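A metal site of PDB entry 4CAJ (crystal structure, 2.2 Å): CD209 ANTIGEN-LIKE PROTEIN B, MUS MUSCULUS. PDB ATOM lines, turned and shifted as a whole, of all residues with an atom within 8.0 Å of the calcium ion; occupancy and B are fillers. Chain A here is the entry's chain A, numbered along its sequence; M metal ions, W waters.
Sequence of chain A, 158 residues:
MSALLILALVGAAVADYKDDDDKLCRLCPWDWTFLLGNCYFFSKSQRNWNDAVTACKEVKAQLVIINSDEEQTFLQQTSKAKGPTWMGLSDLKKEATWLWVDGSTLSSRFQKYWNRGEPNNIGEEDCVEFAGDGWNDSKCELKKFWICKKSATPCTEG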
ATOM      1  N   TRP A 114     -27.238  22.701  -4.277  1.00  0.00           N
ATOM      2  CA  TRP A 114     -28.289  22.865  -5.261  1.00  0.00           C
ATOM      3  C   TRP A 114     -29.599  23.014  -4.521  1.00  0.00           C
ATOM      4  O   TRP A 114     -29.880  22.279  -3.560  1.00  0.00           O
ATOM      5  CB  TRP A 114     -28.360  21.691  -6.183  1.00  0.00           C
ATOM      6  CG  TRP A 114     -27.209  21.548  -7.066  1.00  0.00           C
ATOM      7  CD1 TRP A 114     -26.223  20.615  -6.986  1.00  0.00           C
ATOM      8  CD2 TRP A 114     -26.912  22.358  -8.198  1.00  0.00           C
ATOM      9  NE1 TRP A 114     -25.330  20.777  -8.011  1.00  0.00           N
ATOM     10  CE2 TRP A 114     -25.738  21.848  -8.775  1.00  0.00           C
ATOM     11  CE3 TRP A 114     -27.537  23.449  -8.796  1.00  0.00           C
ATOM     12  CZ2 TRP A 114     -25.167  22.397  -9.898  1.00  0.00           C
ATOM     13  CZ3 TRP A 114     -26.986  23.991  -9.899  1.00  0.00           C
ATOM     14  CH2 TRP A 114     -25.805  23.467 -10.448  1.00  0.00           C
ATOM     15  N   GLY A 117     -34.835  20.908  -7.111  1.00  0.00           N
ATOM     16  CA  GLY A 117     -35.260  21.162  -8.472  1.00  0.00           C
ATOM     17  C   GLY A 117     -34.160  21.812  -9.290  1.00  0.00           C
ATOM     18  O   GLY A 117     -34.422  22.352 -10.362  1.00  0.00           O
ATOM     19  N   GLU A 118     -32.953  21.802  -8.741  1.00  0.00           N
ATOM     20  CA  GLU A 118     -31.769  22.257  -9.463  1.00  0.00           C
ATOM     21  C   GLU A 118     -30.695  21.179  -9.362  1.00  0.00           C
ATOM     22  O   GLU A 118     -30.581  20.520  -8.356  1.00  0.00           O
ATOM     23  CB  GLU A 118     -31.285  23.590  -8.893  1.00  0.00           C
ATOM     24  CG  GLU A 118     -32.336  24.659  -8.950  1.00  0.00           C
ATOM     25  CD  GLU A 118     -32.401  25.273 -10.304  1.00  0.00           C
ATOM     26  OE1 GLU A 118     -31.382  25.214 -11.010  1.00  0.00           O
ATOM     27  OE2 GLU A 118     -33.460  25.779 -10.676  1.00  0.00           O
ATOM     28  N   PRO A 119     -29.873  21.034 -10.402  1.00  0.00           N
ATOM     29  CA  PRO A 119     -29.874  21.748 -11.665  1.00  0.00           C
ATOM     30  C   PRO A 119     -30.958  21.264 -12.579  1.00  0.00           C
ATOM     31  O   PRO A 119     -31.291  20.078 -12.522  1.00  0.00           O
ATOM     32  CB  PRO A 119     -28.500  21.422 -12.254  1.00  0.00           C
ATOM     33  CG  PRO A 119     -28.139  20.141 -11.670  1.00  0.00           C
ATOM     34  CD  PRO A 119     -28.794  20.034 -10.340  1.00  0.00           C
ATOM     35  N   ASN A 120     -31.568  22.153 -13.354  1.00  0.00           N
ATOM     36  CA  ASN A 120     -32.549  21.740 -14.345  1.00  0.00           C
ATOM     37  C   ASN A 120     -32.196  22.317 -15.707  1.00  0.00           C
ATOM     38  O   ASN A 120     -31.057  22.715 -15.932  1.00  0.00           O
ATOM     39  CB  ASN A 120     -33.944  22.158 -13.937  1.00  0.00           C
ATOM     40  CG  ASN A 120     -34.074  23.629 -13.822  1.00  0.00           C
ATOM     41  OD1 ASN A 120     -33.095  24.350 -13.908  1.00  0.00           O
ATOM     42  ND2 ASN A 120     -35.282  24.091 -13.592  1.00  0.00           N
ATOM     43  N   ASN A 121     -33.171  22.327 -16.612  1.00  0.00           N
ATOM     44  CA  ASN A 121     -33.036  22.881 -17.958  1.00  0.00           C
ATOM     45  C   ASN A 121     -31.628  22.636 -18.523  1.00  0.00           C
ATOM     46  O   ASN A 121     -30.988  23.553 -19.055  1.00  0.00           O
ATOM     47  CB  ASN A 121     -33.360  24.374 -17.972  1.00  0.00           C
ATOM     48  CG  ASN A 121     -34.786  24.688 -17.493  1.00  0.00           C
ATOM     49  OD1 ASN A 121     -34.973  25.419 -16.520  1.00  0.00           O
ATOM     50  ND2 ASN A 121     -35.791  24.096 -18.139  1.00  0.00           N
ATOM     51  N   ILE A 122     -31.136  21.414 -18.348  1.00  0.00           N
ATOM     52  CA  ILE A 122     -29.778  21.051 -18.722  1.00  0.00           C
ATOM     53  C   ILE A 122     -29.532  21.286 -20.202  1.00  0.00           C
ATOM     54  O   ILE A 122     -30.350  20.978 -21.063  1.00  0.00           O
ATOM     55  CB  ILE A 122     -29.467  19.602 -18.325  1.00  0.00           C
ATOM     56  CG1 ILE A 122     -29.347  19.494 -16.821  1.00  0.00           C
ATOM     57  CG2 ILE A 122     -28.153  19.141 -18.893  1.00  0.00           C
ATOM     58  CD1 ILE A 122     -29.367  18.074 -16.270  1.00  0.00           C
ATOM     59  N   GLU A 125     -29.392  26.025 -19.524  1.00  0.00           N
ATOM     60  CA  GLU A 125     -28.964  26.912 -18.436  1.00  0.00           C
ATOM     61  C   GLU A 125     -27.640  26.415 -17.927  1.00  0.00           C
ATOM     62  O   GLU A 125     -27.601  25.521 -17.094  1.00  0.00           O
ATOM     63  CB  GLU A 125     -29.986  26.929 -17.274  1.00  0.00           C
ATOM     64  CG  GLU A 125     -31.311  27.651 -17.589  1.00  0.00           C
ATOM     65  CD  GLU A 125     -32.373  27.498 -16.486  1.00  0.00           C
ATOM     66  OE1 GLU A 125     -32.270  26.549 -15.662  1.00  0.00           O
ATOM     67  OE2 GLU A 125     -33.269  28.365 -16.416  1.00  0.00           O
ATOM     68  N   CYS A 127     -24.872  28.072 -16.450  1.00  0.00           N
ATOM     69  CA  CYS A 127     -24.050  28.681 -15.410  1.00  0.00           C
ATOM     70  C   CYS A 127     -24.757  28.706 -14.075  1.00  0.00           C
ATOM     71  O   CYS A 127     -25.989  28.802 -13.999  1.00  0.00           O
ATOM     72  CB  CYS A 127     -23.667  30.110 -15.801  1.00  0.00           C
ATOM     73  SG  CYS A 127     -22.695  30.126 -17.320  1.00  0.00           S
ATOM     74  N   GLU A 129     -25.550  30.218 -10.230  1.00  0.00           N
ATOM     75  CA  GLU A 129     -25.787  31.428  -9.433  1.00  0.00           C
ATOM     76  C   GLU A 129     -26.166  31.132  -7.958  1.00  0.00           C
ATOM     77  O   GLU A 129     -26.730  30.088  -7.661  1.00  0.00           O
ATOM     78  CB  GLU A 129     -26.930  32.232 -10.062  1.00  0.00           C
ATOM     79  CG  GLU A 129     -28.233  31.516  -9.894  1.00  0.00           C
ATOM     80  CD  GLU A 129     -29.442  32.276 -10.402  1.00  0.00           C
ATOM     81  OE1 GLU A 129     -29.260  33.363 -10.945  1.00  0.00           O
ATOM     82  OE2 GLU A 129     -30.594  31.820 -10.172  1.00  0.00           O
ATOM     83  N   TRP A 135     -28.187  26.942  -4.743  1.00  0.00           N
ATOM     84  CA  TRP A 135     -27.714  27.266  -6.083  1.00  0.00           C
ATOM     85  C   TRP A 135     -28.725  26.874  -7.145  1.00  0.00           C
ATOM     86  O   TRP A 135     -29.287  25.806  -7.100  1.00  0.00           O
ATOM     87  CB  TRP A 135     -26.416  26.538  -6.390  1.00  0.00           C
ATOM     88  CG  TRP A 135     -25.315  26.670  -5.388  1.00  0.00           C
ATOM     89  CD1 TRP A 135     -25.261  27.503  -4.316  1.00  0.00           C
ATOM     90  CD2 TRP A 135     -24.102  25.925  -5.371  1.00  0.00           C
ATOM     91  NE1 TRP A 135     -24.076  27.340  -3.646  1.00  0.00           N
ATOM     92  CE2 TRP A 135     -23.346  26.367  -4.283  1.00  0.00           C
ATOM     93  CE3 TRP A 135     -23.580  24.912  -6.173  1.00  0.00           C
ATOM     94  CZ2 TRP A 135     -22.110  25.846  -3.969  1.00  0.00           C
ATOM     95  CZ3 TRP A 135     -22.345  24.404  -5.875  1.00  0.00           C
ATOM     96  CH2 TRP A 135     -21.631  24.862  -4.785  1.00  0.00           C
ATOM     97  N   ASN A 136     -28.908  27.746  -8.132  1.00  0.00           N
ATOM     98  CA  ASN A 136     -29.587  27.461  -9.391  1.00  0.00           C
ATOM     99  C   ASN A 136     -28.664  27.448 -10.559  1.00  0.00           C
ATOM    100  O   ASN A 136     -27.573  28.041 -10.521  1.00  0.00           O
ATOM    101  CB  ASN A 136     -30.643  28.512  -9.695  1.00  0.00           C
ATOM    102  CG  ASN A 136     -31.782  28.456  -8.780  1.00  0.00           C
ATOM    103  OD1 ASN A 136     -31.758  27.693  -7.816  1.00  0.00           O
ATOM    104  ND2 ASN A 136     -32.825  29.250  -9.048  1.00  0.00           N
ATOM    105  N   ASP A 137     -29.097  26.796 -11.623  1.00  0.00           N
ATOM    106  CA  ASP A 137     -28.508  27.040 -12.930  1.00  0.00           C
ATOM    107  C   ASP A 137     -29.375  27.995 -13.744  1.00  0.00           C
ATOM    108  O   ASP A 137     -30.589  28.066 -13.548  1.00  0.00           O
ATOM    109  CB  ASP A 137     -28.282  25.727 -13.668  1.00  0.00           C
ATOM    110  CG  ASP A 137     -29.543  24.954 -13.935  1.00  0.00           C
ATOM    111  OD1 ASP A 137     -30.673  25.281 -13.470  1.00  0.00           O
ATOM    112  OD2 ASP A 137     -29.352  23.952 -14.651  1.00  0.00           O
ATOM    113  N   SER A 138     -28.718  28.783 -14.600  1.00  0.00           N
ATOM    114  CA  SER A 138     -29.374  29.881 -15.319  1.00  0.00           C
ATOM    115  C   SER A 138     -28.786  30.055 -16.721  1.00  0.00           C
ATOM    116  O   SER A 138     -27.672  29.634 -16.991  1.00  0.00           O
ATOM    117  CB  SER A 138     -29.211  31.200 -14.553  1.00  0.00           C
ATOM    118  OG  SER A 138     -29.754  31.131 -13.248  1.00  0.00           O
ATOM    119  N   LYS A 139     -29.535  30.727 -17.589  1.00  0.00           N
ATOM    120  CA  LYS A 139     -28.999  31.097 -18.907  1.00  0.00           C
ATOM    121  C   LYS A 139     -27.777  31.992 -18.734  1.00  0.00           C
ATOM    122  O   LYS A 139     -27.837  33.042 -18.087  1.00  0.00           O
ATOM    123  CB  LYS A 139     -30.052  31.785 -19.763  1.00  0.00           C
ATOM    124  CG  LYS A 139     -31.118  30.844 -20.315  1.00  0.00           C
ATOM    125  CD  LYS A 139     -31.990  31.481 -21.399  1.00  0.00           C
ATOM    126  CE  LYS A 139     -33.033  32.423 -20.839  1.00  0.00           C
ATOM    127  NZ  LYS A 139     -33.910  32.973 -21.916  1.00  0.00           N
HETATM  128 CA    CA M   1     -33.026  26.618 -13.258  1.00  0.00          CA
HETATM  129  O   HOH W   1     -35.315  27.567 -13.737  1.00  0.00           O
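The side-chain carboxylate of Glu 125 sits close to the side-chain amide oxygen of Asn 121, at 3.4 Å.
The side-chain amide oxygen (OD1) of Asn 121 lies within hydrogen-bond range of the side-chain amide nitrogen (ND2) of Asn 120 (3.2 Å).
Merely in contact with the calcium ion: Asn 121 (3.98 Å).
The calcium ion is bound by OD1 of Asn 120 (2.4 Å), OE1 of Glu 125 (2.5 Å), water W1 (2.5 Å), OD1 of Asp 137 (2.7 Å), OE2 of Glu 118 (2.7 Å) and O of Asp 137 (2.8 Å).
The calcium ion has six donor atoms within binding distance.
Slightly farther from the calcium ion lies the side-chain carboxylate (OE1) of Glu 118 (3.1 Å).
Water W1 lies within hydrogen-bond range of the side-chain carboxylate (OE2) of Glu 125 (3.5 Å) and the side-chain amide nitrogen (ND2) of Asn 120 (3.5 Å).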
